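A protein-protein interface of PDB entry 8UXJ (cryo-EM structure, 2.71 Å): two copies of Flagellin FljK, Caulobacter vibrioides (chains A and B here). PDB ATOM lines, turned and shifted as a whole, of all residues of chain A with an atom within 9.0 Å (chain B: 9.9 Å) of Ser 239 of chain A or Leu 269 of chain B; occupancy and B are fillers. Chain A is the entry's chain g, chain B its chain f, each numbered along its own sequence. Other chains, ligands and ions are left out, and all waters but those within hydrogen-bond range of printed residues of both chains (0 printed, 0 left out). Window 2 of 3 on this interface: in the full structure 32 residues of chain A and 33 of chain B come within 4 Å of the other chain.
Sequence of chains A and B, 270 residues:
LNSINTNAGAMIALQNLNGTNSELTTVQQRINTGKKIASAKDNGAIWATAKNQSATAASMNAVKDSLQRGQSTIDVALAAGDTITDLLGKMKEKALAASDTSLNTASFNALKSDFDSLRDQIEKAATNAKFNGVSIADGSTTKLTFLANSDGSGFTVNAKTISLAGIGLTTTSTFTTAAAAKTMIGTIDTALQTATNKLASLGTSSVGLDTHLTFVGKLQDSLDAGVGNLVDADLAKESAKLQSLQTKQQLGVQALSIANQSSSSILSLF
Hydrophobic or aromatic side chains of chain A within 4 Å of the printed part of chain B: Leu 235 and Ala 236.
Of the 10 printed residues of chain B, 4 touch a printed residue of chain A.
Among the printed residues, 7 pairs touch across the chains.
Among the printed residues, no Asp or Glu carboxylate lies within 4 Å of a Lys or Arg side-chain nitrogen of the other chain.
Ser 239 of chain A touches just these residues of chain B: Leu 269 and Phe 270.
Leu 269 of chain B touches two residues of chain A.
Ala 236 of chain A touches one residue of chain B.
No residue of chain B comes within 4 Å of Leu 242 of chain A.
No residue of chain A comes within 4 Å of Ser 268 of chain B.
Printed residues of chain A within 4 Å of Phe 270 of chain B: Leu 235 (3.7 Å) and Ser 239 (3.3 Å).
Printed residues of chain A within 4 Å of Ile 266 of chain B: Leu 235 (3.6 Å).
Ser 244 of chain A touches none of the printed residues of chain B.
The nearest residue of chain B that does not touch Ser 239 of chain A is Ile 266 of chain B (5.7 Å).
The nearest residue of chain A that does not touch Leu 269 of chain B is Gln 243 of chain A (4.6 Å).
The nearest printed residue of chain A that does not touch Ile 266 of chain B is Ala 236 of chain A (5.3 Å).
The backbone carbonyl oxygen of Leu 235 of chain A lies within hydrogen-bond range of the side-chain hydroxyl of Ser 239 of chain A (3.5 Å).
The side-chain hydroxyl (OG) of Ser 239 of chain A sits close to the backbone carbonyl oxygen (O) of Leu 269 of chain B (3.5 Å).
The side-chain carboxylate (OD2) of Asp 234 of chain A sits at hydrogen-bond distance from the backbone NH (N) of Asn 2 of chain B (3.3 Å).
No position is printed for both chains.
Of the 7 pairs that touch across the chains among the printed residues, none has its exchanged pair printed and touching as well.
Among the printed residues, pairs that only touch across the chains: Ser 239 of chain A with Phe 270 of chain B, Leu 235 of chain A with Ile 266 of chain B, Ala 236 of chain A with Leu 269 of chain B, Leu 235 of chain A with Phe 270 of chain B and Leu 235 of chain A with Asn 2 of chain B.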
ATOM      1  N   LEU A  24      -9.159 -19.970 -15.106  1.00  0.00           N
ATOM      2  CA  LEU A  24      -8.039 -20.855 -14.798  1.00  0.00           C
ATOM      3  C   LEU A  24      -8.493 -22.057 -13.979  1.00  0.00           C
ATOM      4  O   LEU A  24      -8.060 -23.189 -14.232  1.00  0.00           O
ATOM      5  CB  LEU A  24      -6.946 -20.087 -14.056  1.00  0.00           C
ATOM      6  CG  LEU A  24      -5.697 -20.909 -13.746  1.00  0.00           C
ATOM      7  CD1 LEU A  24      -5.044 -21.356 -15.038  1.00  0.00           C
ATOM      8  CD2 LEU A  24      -4.720 -20.124 -12.887  1.00  0.00           C
ATOM      9  N   VAL A  27     -10.237 -24.665 -16.210  1.00  0.00           N
ATOM     10  CA  VAL A  27      -9.255 -25.454 -16.953  1.00  0.00           C
ATOM     11  C   VAL A  27      -8.596 -26.478 -16.036  1.00  0.00           C
ATOM     12  O   VAL A  27      -8.408 -27.644 -16.409  1.00  0.00           O
ATOM     13  CB  VAL A  27      -8.217 -24.531 -17.619  1.00  0.00           C
ATOM     14  CG1 VAL A  27      -7.362 -25.315 -18.589  1.00  0.00           C
ATOM     15  CG2 VAL A  27      -8.924 -23.420 -18.347  1.00  0.00           C
ATOM     16  N   ARG A  30     -10.949 -29.460 -15.521  1.00  0.00           N
ATOM     17  CA  ARG A  30     -10.889 -30.440 -16.602  1.00  0.00           C
ATOM     18  C   ARG A  30      -9.582 -31.224 -16.575  1.00  0.00           C
ATOM     19  O   ARG A  30      -9.568 -32.419 -16.889  1.00  0.00           O
ATOM     20  CB  ARG A  30     -11.104 -29.809 -17.976  1.00  0.00           C
ATOM     21  CG  ARG A  30     -12.497 -29.283 -18.234  1.00  0.00           C
ATOM     22  CD  ARG A  30     -12.559 -28.708 -19.633  1.00  0.00           C
ATOM     23  NE  ARG A  30     -13.871 -28.199 -20.012  1.00  0.00           N
ATOM     24  CZ  ARG A  30     -14.277 -26.953 -19.830  1.00  0.00           C
ATOM     25  NH1 ARG A  30     -13.490 -26.046 -19.282  1.00  0.00           N
ATOM     26  NH2 ARG A  30     -15.498 -26.606 -20.224  1.00  0.00           N
ATOM     27  N   ILE A  31      -8.473 -30.577 -16.203  1.00  0.00           N
ATOM     28  CA  ILE A  31      -7.190 -31.285 -16.181  1.00  0.00           C
ATOM     29  C   ILE A  31      -7.212 -32.419 -15.164  1.00  0.00           C
ATOM     30  O   ILE A  31      -6.868 -33.566 -15.476  1.00  0.00           O
ATOM     31  CB  ILE A  31      -6.037 -30.312 -15.885  1.00  0.00           C
ATOM     32  CG1 ILE A  31      -5.915 -29.271 -16.992  1.00  0.00           C
ATOM     33  CG2 ILE A  31      -4.733 -31.079 -15.724  1.00  0.00           C
ATOM     34  CD1 ILE A  31      -4.992 -28.156 -16.634  1.00  0.00           C
ATOM     35  N   ASP A 234     -10.693 -32.833 -24.037  1.00  0.00           N
ATOM     36  CA  ASP A 234      -9.523 -32.885 -24.909  1.00  0.00           C
ATOM     37  C   ASP A 234      -8.371 -32.168 -24.213  1.00  0.00           C
ATOM     38  O   ASP A 234      -8.342 -30.935 -24.159  1.00  0.00           O
ATOM     39  CB  ASP A 234      -9.833 -32.249 -26.261  1.00  0.00           C
ATOM     40  CG  ASP A 234      -9.065 -32.893 -27.399  1.00  0.00           C
ATOM     41  OD1 ASP A 234      -9.282 -32.493 -28.561  1.00  0.00           O
ATOM     42  OD2 ASP A 234      -8.246 -33.798 -27.134  1.00  0.00           O
ATOM     43  N   LEU A 235      -7.414 -32.941 -23.694  1.00  0.00           N
ATOM     44  CA  LEU A 235      -6.343 -32.370 -22.877  1.00  0.00           C
ATOM     45  C   LEU A 235      -5.392 -31.514 -23.709  1.00  0.00           C
ATOM     46  O   LEU A 235      -4.872 -30.494 -23.227  1.00  0.00           O
ATOM     47  CB  LEU A 235      -5.578 -33.490 -22.171  1.00  0.00           C
ATOM     48  CG  LEU A 235      -6.143 -34.061 -20.864  1.00  0.00           C
ATOM     49  CD1 LEU A 235      -6.170 -32.999 -19.773  1.00  0.00           C
ATOM     50  CD2 LEU A 235      -7.518 -34.677 -21.051  1.00  0.00           C
ATOM     51  N   ALA A 236      -5.142 -31.924 -24.956  1.00  0.00           N
ATOM     52  CA  ALA A 236      -4.218 -31.184 -25.810  1.00  0.00           C
ATOM     53  C   ALA A 236      -4.694 -29.754 -26.014  1.00  0.00           C
ATOM     54  O   ALA A 236      -3.889 -28.814 -26.021  1.00  0.00           O
ATOM     55  CB  ALA A 236      -4.058 -31.895 -27.151  1.00  0.00           C
ATOM     56  N   LYS A 237      -6.003 -29.569 -26.181  1.00  0.00           N
ATOM     57  CA  LYS A 237      -6.563 -28.225 -26.187  1.00  0.00           C
ATOM     58  C   LYS A 237      -6.367 -27.548 -24.836  1.00  0.00           C
ATOM     59  O   LYS A 237      -6.135 -26.337 -24.768  1.00  0.00           O
ATOM     60  CB  LYS A 237      -8.046 -28.285 -26.548  1.00  0.00           C
ATOM     61  CG  LYS A 237      -8.703 -26.930 -26.723  1.00  0.00           C
ATOM     62  CD  LYS A 237     -10.170 -27.086 -27.084  1.00  0.00           C
ATOM     63  CE  LYS A 237     -10.337 -27.613 -28.495  1.00  0.00           C
ATOM     64  NZ  LYS A 237      -9.879 -26.626 -29.508  1.00  0.00           N
ATOM     65  N   GLU A 238      -6.459 -28.320 -23.750  1.00  0.00           N
ATOM     66  CA  GLU A 238      -6.435 -27.735 -22.412  1.00  0.00           C
ATOM     67  C   GLU A 238      -5.085 -27.103 -22.099  1.00  0.00           C
ATOM     68  O   GLU A 238      -5.013 -26.125 -21.345  1.00  0.00           O
ATOM     69  CB  GLU A 238      -6.774 -28.799 -21.369  1.00  0.00           C
ATOM     70  CG  GLU A 238      -8.194 -29.320 -21.473  1.00  0.00           C
ATOM     71  CD  GLU A 238      -9.227 -28.269 -21.147  1.00  0.00           C
ATOM     72  OE1 GLU A 238      -8.942 -27.391 -20.309  1.00  0.00           O
ATOM     73  OE2 GLU A 238     -10.319 -28.312 -21.746  1.00  0.00           O
ATOM     74  N   SER A 239      -4.005 -27.669 -22.643  1.00  0.00           N
ATOM     75  CA  SER A 239      -2.667 -27.175 -22.312  1.00  0.00           C
ATOM     76  C   SER A 239      -2.501 -25.702 -22.677  1.00  0.00           C
ATOM     77  O   SER A 239      -1.976 -24.904 -21.881  1.00  0.00           O
ATOM     78  CB  SER A 239      -1.612 -28.009 -23.037  1.00  0.00           C
ATOM     79  OG  SER A 239      -1.627 -29.356 -22.601  1.00  0.00           O
ATOM     80  N   ALA A 240      -2.933 -25.329 -23.882  1.00  0.00           N
ATOM     81  CA  ALA A 240      -2.749 -23.959 -24.346  1.00  0.00           C
ATOM     82  C   ALA A 240      -3.526 -22.978 -23.485  1.00  0.00           C
ATOM     83  O   ALA A 240      -3.007 -21.916 -23.119  1.00  0.00           O
ATOM     84  CB  ALA A 240      -3.173 -23.839 -25.810  1.00  0.00           C
ATOM     85  N   LYS A 241      -4.772 -23.319 -23.153  1.00  0.00           N
ATOM     86  CA  LYS A 241      -5.574 -22.447 -22.304  1.00  0.00           C
ATOM     87  C   LYS A 241      -4.953 -22.317 -20.923  1.00  0.00           C
ATOM     88  O   LYS A 241      -4.933 -21.224 -20.349  1.00  0.00           O
ATOM     89  CB  LYS A 241      -7.004 -22.974 -22.210  1.00  0.00           C
ATOM     90  CG  LYS A 241      -7.772 -22.866 -23.513  1.00  0.00           C
ATOM     91  CD  LYS A 241      -9.156 -23.465 -23.389  1.00  0.00           C
ATOM     92  CE  LYS A 241     -10.049 -22.608 -22.512  1.00  0.00           C
ATOM     93  NZ  LYS A 241     -10.354 -21.300 -23.153  1.00  0.00           N
ATOM     94  N   LEU A 242      -4.419 -23.417 -20.384  1.00  0.00           N
ATOM     95  CA  LEU A 242      -3.752 -23.352 -19.087  1.00  0.00           C
ATOM     96  C   LEU A 242      -2.608 -22.346 -19.110  1.00  0.00           C
ATOM     97  O   LEU A 242      -2.550 -21.429 -18.275  1.00  0.00           O
ATOM     98  CB  LEU A 242      -3.217 -24.734 -18.712  1.00  0.00           C
ATOM     99  CG  LEU A 242      -2.348 -24.869 -17.459  1.00  0.00           C
ATOM    100  CD1 LEU A 242      -2.903 -24.084 -16.276  1.00  0.00           C
ATOM    101  CD2 LEU A 242      -2.085 -26.321 -17.096  1.00  0.00           C
ATOM    102  N   GLN A 243      -1.700 -22.489 -20.077  1.00  0.00           N
ATOM    103  CA  GLN A 243      -0.522 -21.626 -20.108  1.00  0.00           C
ATOM    104  C   GLN A 243      -0.910 -20.174 -20.363  1.00  0.00           C
ATOM    105  O   GLN A 243      -0.385 -19.251 -19.714  1.00  0.00           O
ATOM    106  CB  GLN A 243       0.456 -22.136 -21.161  1.00  0.00           C
ATOM    107  CG  GLN A 243       1.037 -23.487 -20.796  1.00  0.00           C
ATOM    108  CD  GLN A 243       1.994 -24.020 -21.833  1.00  0.00           C
ATOM    109  OE1 GLN A 243       2.191 -23.412 -22.880  1.00  0.00           O
ATOM    110  NE2 GLN A 243       2.586 -25.176 -21.552  1.00  0.00           N
ATOM    111  N   SER A 244      -1.849 -19.958 -21.285  1.00  0.00           N
ATOM    112  CA  SER A 244      -2.297 -18.607 -21.588  1.00  0.00           C
ATOM    113  C   SER A 244      -2.930 -17.952 -20.370  1.00  0.00           C
ATOM    114  O   SER A 244      -2.706 -16.766 -20.109  1.00  0.00           O
ATOM    115  CB  SER A 244      -3.282 -18.637 -22.754  1.00  0.00           C
ATOM    116  OG  SER A 244      -3.756 -17.340 -23.047  1.00  0.00           O
ATOM    117  N   LEU A 245      -3.733 -18.704 -19.614  1.00  0.00           N
ATOM    118  CA  LEU A 245      -4.389 -18.126 -18.447  1.00  0.00           C
ATOM    119  C   LEU A 245      -3.395 -17.817 -17.337  1.00  0.00           C
ATOM    120  O   LEU A 245      -3.563 -16.831 -16.618  1.00  0.00           O
ATOM    121  CB  LEU A 245      -5.499 -19.045 -17.945  1.00  0.00           C
ATOM    122  CG  LEU A 245      -6.728 -19.021 -18.852  1.00  0.00           C
ATOM    123  CD1 LEU A 245      -7.537 -20.276 -18.679  1.00  0.00           C
ATOM    124  CD2 LEU A 245      -7.577 -17.788 -18.583  1.00  0.00           C
ATOM    125  N   GLN A 246      -2.363 -18.646 -17.162  1.00  0.00           N
ATOM    126  CA  GLN A 246      -1.332 -18.282 -16.185  1.00  0.00           C
ATOM    127  C   GLN A 246      -0.623 -16.986 -16.577  1.00  0.00           C
ATOM    128  O   GLN A 246      -0.395 -16.102 -15.731  1.00  0.00           O
ATOM    129  CB  GLN A 246      -0.323 -19.416 -16.011  1.00  0.00           C
ATOM    130  CG  GLN A 246      -0.950 -20.772 -15.799  1.00  0.00           C
ATOM    131  CD  GLN A 246       0.079 -21.855 -15.565  1.00  0.00           C
ATOM    132  OE1 GLN A 246      -0.039 -22.646 -14.630  1.00  0.00           O
ATOM    133  NE2 GLN A 246       1.090 -21.903 -16.420  1.00  0.00           N
ATOM    134  N   ASN B   2      -8.391 -37.096 -27.661  1.00  0.00           N
ATOM    135  CA  ASN B   2      -7.174 -37.425 -26.914  1.00  0.00           C
ATOM    136  C   ASN B   2      -7.547 -37.494 -25.435  1.00  0.00           C
ATOM    137  O   ASN B   2      -7.264 -36.574 -24.666  1.00  0.00           O
ATOM    138  CB  ASN B   2      -6.078 -36.401 -27.177  1.00  0.00           C
ATOM    139  CG  ASN B   2      -5.531 -36.488 -28.583  1.00  0.00           C
ATOM    140  OD1 ASN B   2      -5.315 -37.577 -29.110  1.00  0.00           O
ATOM    141  ND2 ASN B   2      -5.306 -35.336 -29.201  1.00  0.00           N
ATOM    142  N   ILE B   4      -7.566 -39.427 -21.661  1.00  0.00           N
ATOM    143  CA  ILE B   4      -6.906 -40.362 -20.755  1.00  0.00           C
ATOM    144  C   ILE B   4      -7.869 -41.358 -20.133  1.00  0.00           C
ATOM    145  O   ILE B   4      -7.423 -42.337 -19.523  1.00  0.00           O
ATOM    146  CB  ILE B   4      -6.178 -39.603 -19.631  1.00  0.00           C
ATOM    147  CG1 ILE B   4      -7.181 -38.806 -18.803  1.00  0.00           C
ATOM    148  CG2 ILE B   4      -5.111 -38.690 -20.199  1.00  0.00           C
ATOM    149  CD1 ILE B   4      -6.600 -38.217 -17.553  1.00  0.00           C
ATOM    150  N   SER B 263      -1.807 -43.580 -24.839  1.00  0.00           N
ATOM    151  CA  SER B 263      -2.306 -42.582 -23.895  1.00  0.00           C
ATOM    152  C   SER B 263      -1.209 -41.684 -23.332  1.00  0.00           C
ATOM    153  O   SER B 263      -1.516 -40.594 -22.842  1.00  0.00           O
ATOM    154  CB  SER B 263      -3.042 -43.271 -22.745  1.00  0.00           C
ATOM    155  OG  SER B 263      -2.170 -44.106 -22.004  1.00  0.00           O
ATOM    156  N   SER B 264       0.053 -42.106 -23.398  1.00  0.00           N
ATOM    157  CA  SER B 264       1.131 -41.393 -22.722  1.00  0.00           C
ATOM    158  C   SER B 264       1.514 -40.084 -23.399  1.00  0.00           C
ATOM    159  O   SER B 264       2.268 -39.305 -22.806  1.00  0.00           O
ATOM    160  CB  SER B 264       2.363 -42.289 -22.619  1.00  0.00           C
ATOM    161  OG  SER B 264       2.896 -42.565 -23.902  1.00  0.00           O
ATOM    162  N   SER B 265       1.033 -39.826 -24.617  1.00  0.00           N
ATOM    163  CA  SER B 265       1.447 -38.625 -25.337  1.00  0.00           C
ATOM    164  C   SER B 265       0.989 -37.350 -24.640  1.00  0.00           C
ATOM    165  O   SER B 265       1.622 -36.300 -24.793  1.00  0.00           O
ATOM    166  CB  SER B 265       0.917 -38.667 -26.770  1.00  0.00           C
ATOM    167  OG  SER B 265       1.537 -39.704 -27.511  1.00  0.00           O
ATOM    168  N   ILE B 266      -0.110 -37.414 -23.886  1.00  0.00           N
ATOM    169  CA  ILE B 266      -0.610 -36.229 -23.197  1.00  0.00           C
ATOM    170  C   ILE B 266       0.343 -35.789 -22.091  1.00  0.00           C
ATOM    171  O   ILE B 266       0.448 -34.591 -21.794  1.00  0.00           O
ATOM    172  CB  ILE B 266      -2.029 -36.496 -22.664  1.00  0.00           C
ATOM    173  CG1 ILE B 266      -2.981 -36.759 -23.831  1.00  0.00           C
ATOM    174  CG2 ILE B 266      -2.524 -35.331 -21.835  1.00  0.00           C
ATOM    175  CD1 ILE B 266      -4.329 -37.282 -23.417  1.00  0.00           C
ATOM    176  N   LEU B 267       1.058 -36.733 -21.473  1.00  0.00           N
ATOM    177  CA  LEU B 267       1.987 -36.379 -20.405  1.00  0.00           C
ATOM    178  C   LEU B 267       3.080 -35.439 -20.893  1.00  0.00           C
ATOM    179  O   LEU B 267       3.609 -34.644 -20.109  1.00  0.00           O
ATOM    180  CB  LEU B 267       2.607 -37.640 -19.805  1.00  0.00           C
ATOM    181  CG  LEU B 267       1.907 -38.217 -18.576  1.00  0.00           C
ATOM    182  CD1 LEU B 267       2.695 -39.385 -18.017  1.00  0.00           C
ATOM    183  CD2 LEU B 267       1.727 -37.142 -17.523  1.00  0.00           C
ATOM    184  N   SER B 268       3.436 -35.515 -22.176  1.00  0.00           N
ATOM    185  CA  SER B 268       4.437 -34.606 -22.720  1.00  0.00           C
ATOM    186  C   SER B 268       3.941 -33.165 -22.737  1.00  0.00           C
ATOM    187  O   SER B 268       4.749 -32.233 -22.655  1.00  0.00           O
ATOM    188  CB  SER B 268       4.829 -35.045 -24.129  1.00  0.00           C
ATOM    189  OG  SER B 268       5.452 -36.315 -24.112  1.00  0.00           O
ATOM    190  N   LEU B 269       2.627 -32.961 -22.839  1.00  0.00           N
ATOM    191  CA  LEU B 269       2.069 -31.620 -22.943  1.00  0.00           C
ATOM    192  C   LEU B 269       1.911 -30.925 -21.599  1.00  0.00           C
ATOM    193  O   LEU B 269       1.658 -29.717 -21.574  1.00  0.00           O
ATOM    194  CB  LEU B 269       0.709 -31.673 -23.643  1.00  0.00           C
ATOM    195  CG  LEU B 269       0.647 -32.344 -25.015  1.00  0.00           C
ATOM    196  CD1 LEU B 269      -0.687 -32.068 -25.666  1.00  0.00           C
ATOM    197  CD2 LEU B 269       1.774 -31.863 -25.905  1.00  0.00           C
ATOM    198  N   PHE B 270       2.052 -31.644 -20.492  1.00  0.00           N
ATOM    199  CA  PHE B 270       1.935 -31.034 -19.173  1.00  0.00           C
ATOM    200  C   PHE B 270       3.236 -31.181 -18.394  1.00  0.00           C
ATOM    201  O   PHE B 270       3.940 -30.201 -18.154  1.00  0.00           O
ATOM    202  CB  PHE B 270       0.779 -31.655 -18.385  1.00  0.00           C
ATOM    203  CG  PHE B 270      -0.583 -31.359 -18.955  1.00  0.00           C
ATOM    204  CD1 PHE B 270      -1.207 -30.150 -18.701  1.00  0.00           C
ATOM    205  CD2 PHE B 270      -1.244 -32.294 -19.730  1.00  0.00           C
ATOM    206  CE1 PHE B 270      -2.459 -29.881 -19.214  1.00  0.00           C
ATOM    207  CE2 PHE B 270      -2.496 -32.027 -20.246  1.00  0.00           C
ATOM    208  CZ  PHE B 270      -3.103 -30.820 -19.987  1.00  0.00           C
